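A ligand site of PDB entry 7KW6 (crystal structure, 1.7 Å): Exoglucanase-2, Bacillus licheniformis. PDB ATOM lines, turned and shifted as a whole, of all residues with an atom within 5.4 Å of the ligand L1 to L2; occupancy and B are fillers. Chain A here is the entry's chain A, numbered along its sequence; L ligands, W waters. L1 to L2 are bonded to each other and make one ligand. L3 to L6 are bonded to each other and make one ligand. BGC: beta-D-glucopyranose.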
ATOM      1  N   HIS A  30     -18.492  13.600 -14.065  1.00  0.00           N
ATOM      2  CA  HIS A  30     -17.948  12.397 -14.685  1.00  0.00           C
ATOM      3  C   HIS A  30     -19.056  11.638 -15.402  1.00  0.00           C
ATOM      4  O   HIS A  30     -18.872  11.150 -16.528  1.00  0.00           O
ATOM      5  CB  HIS A  30     -17.288  11.529 -13.607  1.00  0.00           C
ATOM      6  CG  HIS A  30     -16.730  10.260 -14.159  1.00  0.00           C
ATOM      7  ND1 HIS A  30     -15.619  10.219 -14.956  1.00  0.00           N
ATOM      8  CD2 HIS A  30     -17.156   8.975 -14.026  1.00  0.00           C
ATOM      9  CE1 HIS A  30     -15.370   8.971 -15.312  1.00  0.00           C
ATOM     10  NE2 HIS A  30     -16.261   8.176 -14.715  1.00  0.00           N
ATOM     11  N   GLU A  38     -14.083   3.873 -10.790  1.00  0.00           N
ATOM     12  CA  GLU A  38     -13.253   3.329 -11.883  1.00  0.00           C
ATOM     13  C   GLU A  38     -11.975   4.147 -12.106  1.00  0.00           C
ATOM     14  O   GLU A  38     -10.939   3.583 -12.519  1.00  0.00           O
ATOM     15  CB  GLU A  38     -14.072   3.266 -13.207  1.00  0.00           C
ATOM     16  CG  GLU A  38     -14.556   4.613 -13.753  1.00  0.00           C
ATOM     17  CD  GLU A  38     -15.604   4.460 -14.837  1.00  0.00           C
ATOM     18  OE1 GLU A  38     -16.097   3.324 -14.971  1.00  0.00           O
ATOM     19  OE2 GLU A  38     -15.933   5.461 -15.543  1.00  0.00           O
ATOM     20  N   ALA A  39     -12.029   5.455 -11.910  1.00  0.00           N
ATOM     21  CA  ALA A  39     -10.832   6.312 -11.966  1.00  0.00           C
ATOM     22  C   ALA A  39     -11.098   7.482 -11.007  1.00  0.00           C
ATOM     23  O   ALA A  39     -10.356   7.575 -10.014  1.00  0.00           O
ATOM     24  CB  ALA A  39     -10.481   6.728 -13.411  1.00  0.00           C
ATOM     25  N   PRO A  40     -12.134   8.313 -11.198  1.00  0.00           N
ATOM     26  CA  PRO A  40     -12.786   8.920 -10.031  1.00  0.00           C
ATOM     27  C   PRO A  40     -13.523   7.808  -9.314  1.00  0.00           C
ATOM     28  O   PRO A  40     -13.796   6.748  -9.889  1.00  0.00           O
ATOM     29  CB  PRO A  40     -13.750   9.957 -10.626  1.00  0.00           C
ATOM     30  CG  PRO A  40     -14.198   9.288 -11.960  1.00  0.00           C
ATOM     31  CD  PRO A  40     -12.930   8.534 -12.437  1.00  0.00           C
ATOM     32  N   THR A  47     -13.447  15.545 -13.788  1.00  0.00           N
ATOM     33  CA  THR A  47     -12.024  15.403 -14.081  1.00  0.00           C
ATOM     34  C   THR A  47     -11.582  16.449 -15.110  1.00  0.00           C
ATOM     35  O   THR A  47     -12.396  17.009 -15.849  1.00  0.00           O
ATOM     36  CB  THR A  47     -11.729  14.027 -14.678  1.00  0.00           C
ATOM     37  OG1 THR A  47     -12.528  13.878 -15.849  1.00  0.00           O
ATOM     38  CG2 THR A  47     -12.103  12.873 -13.738  1.00  0.00           C
ATOM     39  N   GLU A  49     -10.088  15.496 -17.563  1.00  0.00           N
ATOM     40  CA  GLU A  49     -10.500  14.728 -18.725  1.00  0.00           C
ATOM     41  C   GLU A  49     -11.880  15.182 -19.228  1.00  0.00           C
ATOM     42  O   GLU A  49     -12.045  15.458 -20.408  1.00  0.00           O
ATOM     43  CB  GLU A  49     -10.498  13.237 -18.340  1.00  0.00           C
ATOM     44  CG  GLU A  49     -11.194  12.317 -19.353  1.00  0.00           C
ATOM     45  CD  GLU A  49     -11.275  10.948 -18.721  1.00  0.00           C
ATOM     46  OE1 GLU A  49     -12.266  10.659 -18.023  1.00  0.00           O
ATOM     47  OE2 GLU A  49     -10.291  10.171 -18.875  1.00  0.00           O
ATOM     48  N   TRP A 412      -6.188  -1.952 -20.538  1.00  0.00           N
ATOM     49  CA  TRP A 412      -7.498  -1.519 -20.968  1.00  0.00           C
ATOM     50  C   TRP A 412      -7.429  -1.122 -22.433  1.00  0.00           C
ATOM     51  O   TRP A 412      -6.572  -0.329 -22.804  1.00  0.00           O
ATOM     52  CB  TRP A 412      -7.972  -0.308 -20.131  1.00  0.00           C
ATOM     53  CG  TRP A 412      -9.260   0.219 -20.554  1.00  0.00           C
ATOM     54  CD1 TRP A 412     -10.381  -0.485 -20.797  1.00  0.00           C
ATOM     55  CD2 TRP A 412      -9.591   1.614 -20.746  1.00  0.00           C
ATOM     56  NE1 TRP A 412     -11.417   0.394 -21.142  1.00  0.00           N
ATOM     57  CE2 TRP A 412     -10.953   1.673 -21.123  1.00  0.00           C
ATOM     58  CE3 TRP A 412      -8.850   2.806 -20.652  1.00  0.00           C
ATOM     59  CZ2 TRP A 412     -11.615   2.896 -21.401  1.00  0.00           C
ATOM     60  CZ3 TRP A 412      -9.506   4.041 -20.948  1.00  0.00           C
ATOM     61  CH2 TRP A 412     -10.882   4.066 -21.325  1.00  0.00           C
ATOM     62  N   MET A 415      -6.962   2.558 -23.719  1.00  0.00           N
ATOM     63  CA  MET A 415      -5.659   3.169 -23.951  1.00  0.00           C
ATOM     64  C   MET A 415      -5.023   2.711 -25.282  1.00  0.00           C
ATOM     65  O   MET A 415      -3.879   3.118 -25.565  1.00  0.00           O
ATOM     66  CB  MET A 415      -4.738   2.879 -22.749  1.00  0.00           C
ATOM     67  CG  MET A 415      -5.114   3.773 -21.526  1.00  0.00           C
ATOM     68  SD  MET A 415      -4.704   5.477 -21.978  1.00  0.00           S
ATOM     69  CE  MET A 415      -5.524   6.309 -20.620  1.00  0.00           C
ATOM     70  N   TRP A 418      -7.678   5.683 -27.588  1.00  0.00           N
ATOM     71  CA  TRP A 418      -7.434   7.099 -27.283  1.00  0.00           C
ATOM     72  C   TRP A 418      -6.144   7.645 -27.933  1.00  0.00           C
ATOM     73  O   TRP A 418      -6.212   8.716 -28.598  1.00  0.00           O
ATOM     74  CB  TRP A 418      -7.400   7.267 -25.760  1.00  0.00           C
ATOM     75  CG  TRP A 418      -8.762   7.383 -25.150  1.00  0.00           C
ATOM     76  CD1 TRP A 418      -9.994   7.343 -25.786  1.00  0.00           C
ATOM     77  CD2 TRP A 418      -9.003   7.584 -23.773  1.00  0.00           C
ATOM     78  NE1 TRP A 418     -10.990   7.528 -24.848  1.00  0.00           N
ATOM     79  CE2 TRP A 418     -10.410   7.616 -23.600  1.00  0.00           C
ATOM     80  CE3 TRP A 418      -8.152   7.711 -22.649  1.00  0.00           C
ATOM     81  CZ2 TRP A 418     -11.011   7.881 -22.349  1.00  0.00           C
ATOM     82  CZ3 TRP A 418      -8.735   7.912 -21.384  1.00  0.00           C
ATOM     83  CH2 TRP A 418     -10.169   7.986 -21.244  1.00  0.00           C
ATOM     84  N   ALA A 502     -12.306  -4.975 -24.497  1.00  0.00           N
ATOM     85  CA  ALA A 502     -11.981  -4.165 -23.338  1.00  0.00           C
ATOM     86  C   ALA A 502     -10.594  -4.429 -22.793  1.00  0.00           C
ATOM     87  O   ALA A 502     -10.112  -3.617 -22.012  1.00  0.00           O
ATOM     88  CB  ALA A 502     -12.984  -4.394 -22.195  1.00  0.00           C
ATOM     89  N   ASP A 535     -18.617  -0.905 -24.851  1.00  0.00           N
ATOM     90  CA  ASP A 535     -18.243   0.370 -24.272  1.00  0.00           C
ATOM     91  C   ASP A 535     -18.385   1.453 -25.336  1.00  0.00           C
ATOM     92  O   ASP A 535     -17.632   1.462 -26.303  1.00  0.00           O
ATOM     93  CB  ASP A 535     -16.799   0.263 -23.769  1.00  0.00           C
ATOM     94  CG  ASP A 535     -16.354   1.485 -23.014  1.00  0.00           C
ATOM     95  OD1 ASP A 535     -16.643   2.618 -23.495  1.00  0.00           O
ATOM     96  OD2 ASP A 535     -15.708   1.324 -21.953  1.00  0.00           O
ATOM     97  N   VAL A 538     -15.148   3.899 -25.747  1.00  0.00           N
ATOM     98  CA  VAL A 538     -14.136   3.226 -26.540  1.00  0.00           C
ATOM     99  C   VAL A 538     -14.575   3.109 -28.005  1.00  0.00           C
ATOM    100  O   VAL A 538     -13.779   3.323 -28.917  1.00  0.00           O
ATOM    101  CB  VAL A 538     -13.816   1.862 -25.911  1.00  0.00           C
ATOM    102  CG1 VAL A 538     -12.891   1.037 -26.851  1.00  0.00           C
ATOM    103  CG2 VAL A 538     -13.181   2.091 -24.518  1.00  0.00           C
ATOM    104  N   HIS A 593     -19.883  -5.656 -13.933  1.00  0.00           N
ATOM    105  CA  HIS A 593     -18.753  -5.246 -13.091  1.00  0.00           C
ATOM    106  C   HIS A 593     -18.361  -6.303 -12.060  1.00  0.00           C
ATOM    107  O   HIS A 593     -18.792  -6.203 -10.917  1.00  0.00           O
ATOM    108  CB  HIS A 593     -19.079  -3.914 -12.416  1.00  0.00           C
ATOM    109  CG  HIS A 593     -18.881  -2.761 -13.347  1.00  0.00           C
ATOM    110  ND1 HIS A 593     -17.630  -2.249 -13.616  1.00  0.00           N
ATOM    111  CD2 HIS A 593     -19.747  -2.120 -14.174  1.00  0.00           C
ATOM    112  CE1 HIS A 593     -17.735  -1.317 -14.554  1.00  0.00           C
ATOM    113  NE2 HIS A 593     -19.007  -1.203 -14.883  1.00  0.00           N
ATOM    114  N   ARG A 683     -21.641   8.338 -19.260  1.00  0.00           N
ATOM    115  CA  ARG A 683     -20.439   9.065 -18.871  1.00  0.00           C
ATOM    116  C   ARG A 683     -20.261  10.257 -19.799  1.00  0.00           C
ATOM    117  O   ARG A 683     -20.477  10.134 -21.006  1.00  0.00           O
ATOM    118  CB  ARG A 683     -19.210   8.171 -18.965  1.00  0.00           C
ATOM    119  CG  ARG A 683     -19.205   6.965 -18.031  1.00  0.00           C
ATOM    120  CD  ARG A 683     -18.067   6.025 -18.468  1.00  0.00           C
ATOM    121  NE  ARG A 683     -17.856   4.899 -17.522  1.00  0.00           N
ATOM    122  CZ  ARG A 683     -18.450   3.732 -17.647  1.00  0.00           C
ATOM    123  NH1 ARG A 683     -19.316   3.512 -18.636  1.00  0.00           N
ATOM    124  NH2 ARG A 683     -18.195   2.763 -16.764  1.00  0.00           N
ATOM    125  N   TRP A 685     -17.457  11.860 -20.898  1.00  0.00           N
ATOM    126  CA  TRP A 685     -16.446  11.720 -21.953  1.00  0.00           C
ATOM    127  C   TRP A 685     -16.887  10.690 -22.972  1.00  0.00           C
ATOM    128  O   TRP A 685     -16.726  10.893 -24.179  1.00  0.00           O
ATOM    129  CB  TRP A 685     -15.065  11.331 -21.343  1.00  0.00           C
ATOM    130  CG  TRP A 685     -14.899   9.900 -20.947  1.00  0.00           C
ATOM    131  CD1 TRP A 685     -14.948   9.396 -19.657  1.00  0.00           C
ATOM    132  CD2 TRP A 685     -14.595   8.781 -21.778  1.00  0.00           C
ATOM    133  NE1 TRP A 685     -14.693   8.069 -19.656  1.00  0.00           N
ATOM    134  CE2 TRP A 685     -14.467   7.647 -20.936  1.00  0.00           C
ATOM    135  CE3 TRP A 685     -14.427   8.628 -23.166  1.00  0.00           C
ATOM    136  CZ2 TRP A 685     -14.252   6.363 -21.414  1.00  0.00           C
ATOM    137  CZ3 TRP A 685     -14.194   7.336 -23.654  1.00  0.00           C
ATOM    138  CH2 TRP A 685     -14.064   6.224 -22.757  1.00  0.00           C
ATOM    139  N   SER A 686     -17.544   9.630 -22.524  1.00  0.00           N
ATOM    140  CA  SER A 686     -17.956   8.587 -23.461  1.00  0.00           C
ATOM    141  C   SER A 686     -18.978   9.111 -24.448  1.00  0.00           C
ATOM    142  O   SER A 686     -18.925   8.779 -25.627  1.00  0.00           O
ATOM    143  CB  SER A 686     -18.560   7.423 -22.692  1.00  0.00           C
ATOM    144  OG  SER A 686     -17.659   7.111 -21.665  1.00  0.00           O
HETATM  145  C2  BGC L   1     -12.467   0.247 -17.719  1.00  0.00           C
HETATM  146  C3  BGC L   1     -12.388   1.571 -17.050  1.00  0.00           C
HETATM  147  C4  BGC L   1     -13.110   2.667 -17.856  1.00  0.00           C
HETATM  148  C5  BGC L   1     -14.565   2.206 -18.081  1.00  0.00           C
HETATM  149  C6  BGC L   1     -15.386   3.152 -18.920  1.00  0.00           C
HETATM  150  C1  BGC L   1     -13.952  -0.055 -17.839  1.00  0.00           C
HETATM  151  O1  BGC L   1     -14.095  -1.244 -18.393  1.00  0.00           O
HETATM  152  O2  BGC L   1     -11.933  -0.770 -16.869  1.00  0.00           O
HETATM  153  O3  BGC L   1     -10.990   1.895 -16.769  1.00  0.00           O
HETATM  154  O4  BGC L   1     -13.166   3.846 -17.041  1.00  0.00           O
HETATM  155  O5  BGC L   1     -14.445   0.953 -18.833  1.00  0.00           O
HETATM  156  O6  BGC L   1     -14.794   3.316 -20.218  1.00  0.00           O
HETATM  157  C2  BGC L   2     -12.815   6.191 -16.947  1.00  0.00           C
HETATM  158  C3  BGC L   2     -11.877   7.310 -17.388  1.00  0.00           C
HETATM  159  C4  BGC L   2     -10.433   6.965 -17.122  1.00  0.00           C
HETATM  160  C5  BGC L   2     -10.112   5.662 -17.845  1.00  0.00           C
HETATM  161  C6  BGC L   2      -8.692   5.188 -17.659  1.00  0.00           C
HETATM  162  C1  BGC L   2     -12.432   4.893 -17.634  1.00  0.00           C
HETATM  163  O2  BGC L   2     -14.190   6.470 -17.274  1.00  0.00           O
HETATM  164  O3  BGC L   2     -12.255   8.476 -16.609  1.00  0.00           O
HETATM  165  O4  BGC L   2      -9.591   8.031 -17.644  1.00  0.00           O
HETATM  166  O5  BGC L   2     -11.023   4.641 -17.317  1.00  0.00           O
HETATM  167  O6  BGC L   2      -8.372   5.161 -16.258  1.00  0.00           O
HETATM  168  C2  BGC L   3      -4.682   9.134 -12.830  1.00  0.00           C
HETATM  169  C3  BGC L   3      -4.139   9.399 -11.451  1.00  0.00           C
HETATM  170  C4  BGC L   3      -3.462  10.697 -11.251  1.00  0.00           C
HETATM  171  C5  BGC L   3      -4.297  11.839 -11.806  1.00  0.00           C
HETATM  172  C6  BGC L   3      -3.496  13.113 -11.975  1.00  0.00           C
HETATM  173  C1  BGC L   3      -5.495  10.309 -13.310  1.00  0.00           C
HETATM  174  O1  BGC L   3      -5.779  10.096 -14.637  1.00  0.00           O
HETATM  175  O2  BGC L   3      -5.503   7.931 -12.899  1.00  0.00           O
HETATM  176  O3  BGC L   3      -3.254   8.344 -11.073  1.00  0.00           O
HETATM  177  O4  BGC L   3      -3.382  10.855  -9.814  1.00  0.00           O
HETATM  178  O5  BGC L   3      -4.697  11.510 -13.172  1.00  0.00           O
HETATM  179  O6  BGC L   3      -2.297  12.784 -12.671  1.00  0.00           O
HETATM  180  C2  BGC L   4      -2.268  12.171  -8.058  1.00  0.00           C
HETATM  181  C3  BGC L   4      -0.889  12.608  -7.674  1.00  0.00           C
HETATM  182  C4  BGC L   4       0.066  11.466  -7.466  1.00  0.00           C
HETATM  183  C5  BGC L   4       0.019  10.512  -8.662  1.00  0.00           C
HETATM  184  C6  BGC L   4       0.770   9.228  -8.354  1.00  0.00           C
HETATM  185  C1  BGC L   4      -2.129  11.308  -9.345  1.00  0.00           C
HETATM  186  O2  BGC L   4      -3.017  13.373  -8.405  1.00  0.00           O
HETATM  187  O3  BGC L   4      -0.903  13.509  -6.536  1.00  0.00           O
HETATM  188  O4  BGC L   4       1.430  11.894  -7.428  1.00  0.00           O
HETATM  189  O5  BGC L   4      -1.363  10.115  -8.924  1.00  0.00           O
HETATM  190  O6  BGC L   4       0.520   8.316  -9.438  1.00  0.00           O
HETATM  191  C2  BGC L   5       3.408  12.161  -6.199  1.00  0.00           C
HETATM  192  C3  BGC L   5       3.965  12.506  -4.878  1.00  0.00           C
HETATM  193  C4  BGC L   5       3.471  13.845  -4.414  1.00  0.00           C
HETATM  194  C5  BGC L   5       1.939  13.929  -4.467  1.00  0.00           C
HETATM  195  C6  BGC L   5       1.438  15.374  -4.391  1.00  0.00           C
HETATM  196  C1  BGC L   5       1.898  12.116  -6.151  1.00  0.00           C
HETATM  197  O2  BGC L   5       3.918  10.885  -6.654  1.00  0.00           O
HETATM  198  O3  BGC L   5       5.442  12.569  -4.959  1.00  0.00           O
HETATM  199  O4  BGC L   5       3.863  14.010  -3.011  1.00  0.00           O
HETATM  200  O5  BGC L   5       1.408  13.446  -5.759  1.00  0.00           O
HETATM  201  O6  BGC L   5       0.039  15.368  -4.106  1.00  0.00           O
HETATM  202  C2  BGC L   6       4.378  15.569  -1.300  1.00  0.00           C
HETATM  203  C3  BGC L   6       5.106  16.782  -0.942  1.00  0.00           C
HETATM  204  C4  BGC L   6       6.536  16.695  -1.337  1.00  0.00           C
HETATM  205  C5  BGC L   6       6.697  16.384  -2.870  1.00  0.00           C
HETATM  206  C6  BGC L   6       8.067  16.170  -3.232  1.00  0.00           C
HETATM  207  C1  BGC L   6       4.503  15.267  -2.767  1.00  0.00           C
HETATM  208  O2  BGC L   6       2.922  15.714  -0.989  1.00  0.00           O
HETATM  209  O3  BGC L   6       5.052  16.943   0.556  1.00  0.00           O
HETATM  210  O4  BGC L   6       7.207  17.925  -1.055  1.00  0.00           O
HETATM  211  O5  BGC L   6       5.910  15.126  -3.140  1.00  0.00           O
HETATM  212  O6  BGC L   6       8.529  14.871  -2.842  1.00  0.00           O
HETATM  213  O   HOH W   1     -13.968  -0.753 -21.825  1.00  0.00           O
HETATM  214  O   HOH W   2      -9.304   3.100 -14.813  1.00  0.00           O
HETATM  215  O   HOH W   3      -7.219   6.187 -13.967  1.00  0.00           O
HETATM  216  O   HOH W   4      -6.596   8.664 -18.475  1.00  0.00           O
HETATM  217  O   HOH W   5     -16.912   4.475 -21.712  1.00  0.00           O
HETATM  218  O   HOH W   6     -13.722  -1.898 -14.664  1.00  0.00           O
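His 30 touches the ligand L1 to L2. CB of Ala 39 touches C4 of BGC L2, at 3.7 Å. CZ2 of Trp 412 touches O6 of BGC L1, 3.4 Å away. Trp 418 touches the ligand L1 to L2. NE of Arg 683 touches C6 of BGC L1, 3.3 Å away. Hydrophobic or aromatic side chains that line the ligand L1 to L2: His 30, Ala 39, Trp 412, Trp 418 and Trp 685. Within 4 Å of the ligand L1 to L2: His 30, Glu 38, Ala 39, Glu 49, Trp 412, Trp 418, Asp 535, Arg 683 and Trp 685.
Water W2 bridges an oxygen (O6) of BGC L2 (2.7 Å) and the backbone carbonyl oxygen of Glu 38 (2.9 Å). Water W3 lies within hydrogen-bond range of O2 of BGC L3 (2.7 Å) and O6 of BGC L2 (2.8 Å). Water W5 lies within hydrogen-bond range of the side-chain carboxylate (OD1) of Asp 535 (2.6 Å), the side-chain hydroxyl (OG) of Ser 686 (2.7 Å) and an oxygen (O6) of BGC L1 (2.8 Å). Water W1 lies within hydrogen-bond range of OD2 of Asp 535 (2.7 Å), NE1 of Trp 412 (2.9 Å) and O1 of BGC L1 (3.5 Å).
The backbone NH (N) of Glu 49 lies close to the side-chain hydroxyl (OG1) of Thr 47 (3.4 Å). OE2 of Glu 38 is in hydrogen-bond range of NE2 of His 30 (2.9 Å). The side-chain carboxylate of Glu 38 is in salt-bridge range of the guanidinium group of Arg 683 (2.8 Å). The side-chain carboxylate (OD1) of Asp 535 is in hydrogen-bond range of the backbone NH (N) of Val 538.
The side-chain carboxylate of Glu 49 lies within hydrogen-bond range of an oxygen (O4) of BGC L2, 2.6 Å away. The side-chain carboxylate of Glu 38 sits at hydrogen-bond distance from an oxygen (O2) of BGC L2 (2.7 Å). An oxygen (O2) of BGC L2 lies within hydrogen-bond range of the indole nitrogen (NE1) of Trp 685, 2.9 Å away. The side-chain carboxylate (OD2) of Asp 535 lies within hydrogen-bond range of an oxygen (O6) of BGC L1.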
